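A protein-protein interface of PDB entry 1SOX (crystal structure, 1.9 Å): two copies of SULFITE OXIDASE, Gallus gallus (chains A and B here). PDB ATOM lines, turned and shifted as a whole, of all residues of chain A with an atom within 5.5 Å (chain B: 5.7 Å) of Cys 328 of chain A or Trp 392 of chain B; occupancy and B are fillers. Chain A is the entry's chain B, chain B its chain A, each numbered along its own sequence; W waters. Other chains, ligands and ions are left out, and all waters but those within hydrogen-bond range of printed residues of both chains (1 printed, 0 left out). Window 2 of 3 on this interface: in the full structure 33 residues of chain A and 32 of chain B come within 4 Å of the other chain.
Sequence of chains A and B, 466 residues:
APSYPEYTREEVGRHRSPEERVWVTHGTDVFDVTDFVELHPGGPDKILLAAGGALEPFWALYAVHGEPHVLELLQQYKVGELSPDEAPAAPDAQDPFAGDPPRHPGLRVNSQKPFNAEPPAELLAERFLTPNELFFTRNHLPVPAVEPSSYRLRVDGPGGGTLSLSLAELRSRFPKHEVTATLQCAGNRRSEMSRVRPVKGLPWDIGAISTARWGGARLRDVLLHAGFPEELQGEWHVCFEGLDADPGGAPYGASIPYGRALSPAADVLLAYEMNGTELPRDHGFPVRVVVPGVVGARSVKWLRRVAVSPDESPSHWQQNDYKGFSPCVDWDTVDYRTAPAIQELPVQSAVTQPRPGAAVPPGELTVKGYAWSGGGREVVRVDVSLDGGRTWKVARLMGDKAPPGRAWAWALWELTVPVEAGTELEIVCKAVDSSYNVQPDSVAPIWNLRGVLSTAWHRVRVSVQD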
ATOM      1  N   SER A 326      10.316 -10.407  21.870  1.00  0.00           N
ATOM      2  CA  SER A 326      10.011 -11.664  21.172  1.00  0.00           C
ATOM      3  C   SER A 326      10.387 -12.809  22.079  1.00  0.00           C
ATOM      4  O   SER A 326      11.354 -12.742  22.860  1.00  0.00           O
ATOM      5  CB  SER A 326      10.842 -11.662  19.886  1.00  0.00           C
ATOM      6  OG  SER A 326      10.620 -12.866  19.187  1.00  0.00           O
ATOM      7  N   PRO A 327       9.711 -13.942  21.971  1.00  0.00           N
ATOM      8  CA  PRO A 327       9.974 -15.116  22.779  1.00  0.00           C
ATOM      9  C   PRO A 327      11.363 -15.706  22.522  1.00  0.00           C
ATOM     10  O   PRO A 327      11.850 -16.454  23.361  1.00  0.00           O
ATOM     11  CB  PRO A 327       8.863 -16.132  22.479  1.00  0.00           C
ATOM     12  CG  PRO A 327       8.253 -15.591  21.218  1.00  0.00           C
ATOM     13  CD  PRO A 327       8.566 -14.118  21.070  1.00  0.00           C
ATOM     14  N   CYS A 328      12.017 -15.387  21.439  1.00  0.00           N
ATOM     15  CA  CYS A 328      13.347 -15.814  21.076  1.00  0.00           C
ATOM     16  C   CYS A 328      14.455 -15.080  21.837  1.00  0.00           C
ATOM     17  O   CYS A 328      15.594 -15.539  21.849  1.00  0.00           O
ATOM     18  CB  CYS A 328      13.604 -15.632  19.583  1.00  0.00           C
ATOM     19  SG  CYS A 328      13.638 -13.983  18.856  1.00  0.00           S
ATOM     20  N   VAL A 329      14.160 -13.917  22.401  1.00  0.00           N
ATOM     21  CA  VAL A 329      15.172 -13.122  23.075  1.00  0.00           C
ATOM     22  C   VAL A 329      15.589 -13.747  24.394  1.00  0.00           C
ATOM     23  O   VAL A 329      14.766 -14.214  25.173  1.00  0.00           O
ATOM     24  CB  VAL A 329      14.688 -11.675  23.293  1.00  0.00           C
ATOM     25  CG1 VAL A 329      15.663 -10.891  24.152  1.00  0.00           C
ATOM     26  CG2 VAL A 329      14.505 -10.976  21.945  1.00  0.00           C
ATOM     27  N   ASP A 330      16.902 -13.758  24.627  1.00  0.00           N
ATOM     28  CA  ASP A 330      17.414 -14.285  25.894  1.00  0.00           C
ATOM     29  C   ASP A 330      18.289 -13.228  26.555  1.00  0.00           C
ATOM     30  O   ASP A 330      18.495 -12.151  25.995  1.00  0.00           O
ATOM     31  CB  ASP A 330      18.179 -15.589  25.691  1.00  0.00           C
ATOM     32  CG  ASP A 330      18.072 -16.508  26.888  1.00  0.00           C
ATOM     33  OD1 ASP A 330      17.819 -16.026  28.017  1.00  0.00           O
ATOM     34  OD2 ASP A 330      18.248 -17.735  26.719  1.00  0.00           O
ATOM     35  N   THR A 333      21.031 -11.628  24.412  1.00  0.00           N
ATOM     36  CA  THR A 333      20.682 -10.812  23.264  1.00  0.00           C
ATOM     37  C   THR A 333      19.705  -9.681  23.590  1.00  0.00           C
ATOM     38  O   THR A 333      19.483  -8.810  22.740  1.00  0.00           O
ATOM     39  CB  THR A 333      20.029 -11.651  22.133  1.00  0.00           C
ATOM     40  OG1 THR A 333      18.870 -12.313  22.676  1.00  0.00           O
ATOM     41  CG2 THR A 333      21.004 -12.685  21.590  1.00  0.00           C
ATOM     42  N   ALA A 444       3.567 -20.010  25.721  1.00  0.00           N
ATOM     43  CA  ALA A 444       4.856 -20.051  25.045  1.00  0.00           C
ATOM     44  C   ALA A 444       5.135 -18.991  24.016  1.00  0.00           C
ATOM     45  O   ALA A 444       6.218 -18.380  23.982  1.00  0.00           O
ATOM     46  CB  ALA A 444       5.116 -21.440  24.436  1.00  0.00           C
ATOM     47  N   PRO A 445       4.250 -18.697  23.075  1.00  0.00           N
ATOM     48  CA  PRO A 445       4.438 -17.731  22.024  1.00  0.00           C
ATOM     49  C   PRO A 445       4.470 -16.281  22.526  1.00  0.00           C
ATOM     50  O   PRO A 445       5.007 -15.423  21.822  1.00  0.00           O
ATOM     51  CB  PRO A 445       3.310 -17.943  20.992  1.00  0.00           C
ATOM     52  CG  PRO A 445       2.689 -19.232  21.468  1.00  0.00           C
ATOM     53  CD  PRO A 445       2.943 -19.391  22.961  1.00  0.00           C
ATOM     54  N   ASP B 383       6.799 -11.191  14.655  1.00  0.00           N
ATOM     55  CA  ASP B 383       7.530 -12.420  14.929  1.00  0.00           C
ATOM     56  C   ASP B 383       7.209 -13.400  13.801  1.00  0.00           C
ATOM     57  O   ASP B 383       6.043 -13.474  13.397  1.00  0.00           O
ATOM     58  CB  ASP B 383       7.023 -13.016  16.238  1.00  0.00           C
ATOM     59  CG  ASP B 383       7.445 -12.252  17.483  1.00  0.00           C
ATOM     60  OD1 ASP B 383       8.504 -11.584  17.496  1.00  0.00           O
ATOM     61  OD2 ASP B 383       6.721 -12.334  18.485  1.00  0.00           O
ATOM     62  N   VAL B 384       8.217 -14.096  13.277  1.00  0.00           N
ATOM     63  CA  VAL B 384       8.051 -14.980  12.134  1.00  0.00           C
ATOM     64  C   VAL B 384       8.664 -16.353  12.463  1.00  0.00           C
ATOM     65  O   VAL B 384       9.812 -16.381  12.904  1.00  0.00           O
ATOM     66  CB  VAL B 384       8.802 -14.456  10.909  1.00  0.00           C
ATOM     67  CG1 VAL B 384       8.727 -15.412   9.732  1.00  0.00           C
ATOM     68  CG2 VAL B 384       8.321 -13.088  10.460  1.00  0.00           C
ATOM     69  N   SER B 385       7.886 -17.396  12.263  1.00  0.00           N
ATOM     70  CA  SER B 385       8.252 -18.766  12.550  1.00  0.00           C
ATOM     71  C   SER B 385       8.314 -19.588  11.260  1.00  0.00           C
ATOM     72  O   SER B 385       7.561 -19.303  10.332  1.00  0.00           O
ATOM     73  CB  SER B 385       7.220 -19.429  13.468  1.00  0.00           C
ATOM     74  OG  SER B 385       7.561 -20.807  13.716  1.00  0.00           O
ATOM     75  N   ASP B 387       8.577 -23.088  11.663  1.00  0.00           N
ATOM     76  CA  ASP B 387       8.216 -24.385  12.182  1.00  0.00           C
ATOM     77  C   ASP B 387       6.861 -24.453  12.857  1.00  0.00           C
ATOM     78  O   ASP B 387       6.672 -25.038  13.920  1.00  0.00           O
ATOM     79  CB  ASP B 387       9.314 -24.862  13.141  1.00  0.00           C
ATOM     80  CG  ASP B 387       9.531 -23.956  14.329  1.00  0.00           C
ATOM     81  OD1 ASP B 387       8.697 -23.072  14.611  1.00  0.00           O
ATOM     82  OD2 ASP B 387      10.553 -24.124  15.028  1.00  0.00           O
ATOM     83  N   GLY B 389       5.151 -22.161  14.428  1.00  0.00           N
ATOM     84  CA  GLY B 389       4.948 -21.395  15.638  1.00  0.00           C
ATOM     85  C   GLY B 389       5.651 -21.872  16.891  1.00  0.00           C
ATOM     86  O   GLY B 389       5.273 -21.440  17.981  1.00  0.00           O
ATOM     87  N   ARG B 390       6.649 -22.743  16.768  1.00  0.00           N
ATOM     88  CA  ARG B 390       7.390 -23.240  17.925  1.00  0.00           C
ATOM     89  C   ARG B 390       8.500 -22.236  18.251  1.00  0.00           C
ATOM     90  O   ARG B 390       8.664 -21.862  19.409  1.00  0.00           O
ATOM     91  CB  ARG B 390       8.008 -24.609  17.629  1.00  0.00           C
ATOM     92  CG  ARG B 390       7.041 -25.634  17.063  1.00  0.00           C
ATOM     93  CD  ARG B 390       7.553 -27.067  17.175  1.00  0.00           C
ATOM     94  NE  ARG B 390       6.546 -28.001  16.646  1.00  0.00           N
ATOM     95  CZ  ARG B 390       5.625 -28.557  17.431  1.00  0.00           C
ATOM     96  NH1 ARG B 390       5.591 -28.314  18.737  1.00  0.00           N
ATOM     97  NH2 ARG B 390       4.723 -29.384  16.905  1.00  0.00           N
ATOM     98  N   THR B 391       9.245 -21.846  17.222  1.00  0.00           N
ATOM     99  CA  THR B 391      10.334 -20.890  17.408  1.00  0.00           C
ATOM    100  C   THR B 391      10.176 -19.710  16.472  1.00  0.00           C
ATOM    101  O   THR B 391       9.584 -19.808  15.397  1.00  0.00           O
ATOM    102  CB  THR B 391      11.730 -21.493  17.171  1.00  0.00           C
ATOM    103  OG1 THR B 391      11.818 -21.871  15.799  1.00  0.00           O
ATOM    104  CG2 THR B 391      11.966 -22.692  18.085  1.00  0.00           C
ATOM    105  N   TRP B 392      10.631 -18.533  16.948  1.00  0.00           N
ATOM    106  CA  TRP B 392      10.425 -17.296  16.214  1.00  0.00           C
ATOM    107  C   TRP B 392      11.682 -16.463  16.011  1.00  0.00           C
ATOM    108  O   TRP B 392      12.638 -16.533  16.788  1.00  0.00           O
ATOM    109  CB  TRP B 392       9.438 -16.405  17.032  1.00  0.00           C
ATOM    110  CG  TRP B 392       8.179 -17.112  17.429  1.00  0.00           C
ATOM    111  CD1 TRP B 392       7.992 -17.909  18.522  1.00  0.00           C
ATOM    112  CD2 TRP B 392       6.939 -17.147  16.703  1.00  0.00           C
ATOM    113  NE1 TRP B 392       6.710 -18.419  18.529  1.00  0.00           N
ATOM    114  CE2 TRP B 392       6.061 -17.964  17.416  1.00  0.00           C
ATOM    115  CE3 TRP B 392       6.523 -16.524  15.522  1.00  0.00           C
ATOM    116  CZ2 TRP B 392       4.735 -18.189  17.020  1.00  0.00           C
ATOM    117  CZ3 TRP B 392       5.213 -16.758  15.107  1.00  0.00           C
ATOM    118  CH2 TRP B 392       4.365 -17.572  15.853  1.00  0.00           C
ATOM    119  N   LYS B 393      11.642 -15.642  14.983  1.00  0.00           N
ATOM    120  CA  LYS B 393      12.649 -14.660  14.636  1.00  0.00           C
ATOM    121  C   LYS B 393      11.938 -13.314  14.436  1.00  0.00           C
ATOM    122  O   LYS B 393      10.750 -13.327  14.081  1.00  0.00           O
ATOM    123  CB  LYS B 393      13.406 -15.070  13.375  1.00  0.00           C
ATOM    124  CG  LYS B 393      14.421 -16.181  13.660  1.00  0.00           C
ATOM    125  CD  LYS B 393      14.913 -16.852  12.384  1.00  0.00           C
ATOM    126  CE  LYS B 393      15.318 -18.300  12.664  1.00  0.00           C
ATOM    127  NZ  LYS B 393      16.232 -18.384  13.848  1.00  0.00           N
ATOM    128  N   VAL B 394      12.620 -12.214  14.723  1.00  0.00           N
ATOM    129  CA  VAL B 394      12.004 -10.886  14.571  1.00  0.00           C
ATOM    130  C   VAL B 394      12.213 -10.350  13.179  1.00  0.00           C
ATOM    131  O   VAL B 394      13.327 -10.316  12.640  1.00  0.00           O
ATOM    132  CB  VAL B 394      12.571  -9.929  15.637  1.00  0.00           C
ATOM    133  CG1 VAL B 394      12.051  -8.507  15.480  1.00  0.00           C
ATOM    134  CG2 VAL B 394      12.227 -10.476  17.019  1.00  0.00           C
ATOM    135  N   VAL B 428       4.721 -18.824   9.770  1.00  0.00           N
ATOM    136  CA  VAL B 428       3.707 -18.156  10.569  1.00  0.00           C
ATOM    137  C   VAL B 428       4.187 -16.748  10.946  1.00  0.00           C
ATOM    138  O   VAL B 428       5.365 -16.565  11.245  1.00  0.00           O
ATOM    139  CB  VAL B 428       3.473 -18.917  11.881  1.00  0.00           C
ATOM    140  CG1 VAL B 428       2.349 -18.277  12.701  1.00  0.00           C
ATOM    141  CG2 VAL B 428       3.151 -20.397  11.712  1.00  0.00           C
ATOM    142  N   CYS B 429       3.257 -15.799  10.973  1.00  0.00           N
ATOM    143  CA  CYS B 429       3.654 -14.449  11.424  1.00  0.00           C
ATOM    144  C   CYS B 429       2.634 -14.007  12.462  1.00  0.00           C
ATOM    145  O   CYS B 429       1.464 -14.416  12.435  1.00  0.00           O
ATOM    146  CB  CYS B 429       3.779 -13.435  10.308  1.00  0.00           C
ATOM    147  SG  CYS B 429       2.195 -13.021   9.486  1.00  0.00           S
ATOM    148  N   LYS B 430       3.105 -13.224  13.428  1.00  0.00           N
ATOM    149  CA  LYS B 430       2.176 -12.664  14.419  1.00  0.00           C
ATOM    150  C   LYS B 430       2.715 -11.280  14.780  1.00  0.00           C
ATOM    151  O   LYS B 430       3.938 -11.085  14.781  1.00  0.00           O
ATOM    152  CB  LYS B 430       1.971 -13.534  15.636  1.00  0.00           C
ATOM    153  CG  LYS B 430       3.265 -13.752  16.452  1.00  0.00           C
ATOM    154  CD  LYS B 430       2.955 -14.745  17.573  1.00  0.00           C
ATOM    155  CE  LYS B 430       4.248 -15.068  18.363  1.00  0.00           C
ATOM    156  NZ  LYS B 430       4.545 -13.901  19.259  1.00  0.00           N
ATOM    157  N   TRP B 457      -3.110 -16.386  13.958  1.00  0.00           N
ATOM    158  CA  TRP B 457      -1.893 -16.372  13.164  1.00  0.00           C
ATOM    159  C   TRP B 457      -2.133 -16.911  11.752  1.00  0.00           C
ATOM    160  O   TRP B 457      -2.732 -17.983  11.604  1.00  0.00           O
ATOM    161  CB  TRP B 457      -0.800 -17.213  13.811  1.00  0.00           C
ATOM    162  CG  TRP B 457      -0.554 -16.952  15.270  1.00  0.00           C
ATOM    163  CD1 TRP B 457      -0.805 -15.822  15.994  1.00  0.00           C
ATOM    164  CD2 TRP B 457       0.070 -17.875  16.175  1.00  0.00           C
ATOM    165  NE1 TRP B 457      -0.402 -15.991  17.293  1.00  0.00           N
ATOM    166  CE2 TRP B 457       0.156 -17.245  17.430  1.00  0.00           C
ATOM    167  CE3 TRP B 457       0.553 -19.189  16.042  1.00  0.00           C
ATOM    168  CZ2 TRP B 457       0.699 -17.871  18.542  1.00  0.00           C
ATOM    169  CZ3 TRP B 457       1.085 -19.808  17.155  1.00  0.00           C
ATOM    170  CH2 TRP B 457       1.157 -19.157  18.404  1.00  0.00           C
HETATM  171  O   HOH W   1      11.676 -18.405  19.743  1.00  0.00           O
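Among the printed residues, merely in contact across the chains: Ser 326 of chain A with Val 394 of chain B, Pro 445 of chain A with Trp 457 of chain B, Pro 327 of chain A with Trp 392 of chain B and Pro 327 of chain A with Asp 383 of chain B.
The side-chain amino group of Lys 430 of chain B is in salt-bridge range of the side-chain carboxylate of Asp 383 of chain B (2.8 Å).
O of Gly 389 of chain B lies within hydrogen-bond range of NE1 of Trp 392 of chain B (3.4 Å).
SG of Cys 328 of chain A is in hydrogen-bond range of OG of Ser 326 of chain A (3.2 Å).
No position is printed for both chains.
Of the 7 pairs that touch across the chains among the printed residues, none has its exchanged pair printed and touching as well.
Cys 328 of chain A touches one residue of chain B.
Val 329 of chain A touches none of the printed residues of chain B.
Val 384 of chain B touches none of the printed residues of chain A.
Trp 392 of chain B touches just these residues of chain A: Pro 327 and Cys 328.
Of the printed residues of chain A, Val 394 of chain B touches Ser 326 (3.4 Å).
Printed residues of chain A within 4 Å of Trp 457 of chain B: Pro 445 (3.4 Å).
The side-chain hydroxyl of Ser 326 of chain A is in hydrogen-bond range of the side-chain carboxylate of Asp 383 of chain B, 3.0 Å away.
The backbone carbonyl oxygen (O) of Trp 392 of chain B lies close to the side-chain sulfur (SG) of Cys 328 of chain A, at 3.4 Å.
The side-chain amino group of Lys 430 of chain B is in hydrogen-bond range of the backbone carbonyl oxygen of Pro 445 of chain A, at 3.0 Å.
Water W1 lies within hydrogen-bond range of the backbone NH of Trp 392 of chain B and the backbone NH of Cys 328 of chain A.
Hydrophobic or aromatic side chains of chain A that line the printed part of chain B: Pro 327 and Pro 445.
Hydrophobic or aromatic side chains of chain B that line the printed part of chain A: Trp 392, Val 394 and Trp 457.
Among the printed residues, 7 pairs touch across the chains.
Among the printed residues, no Asp or Glu carboxylate lies within 4 Å of a Lys or Arg side-chain nitrogen of the other chain.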
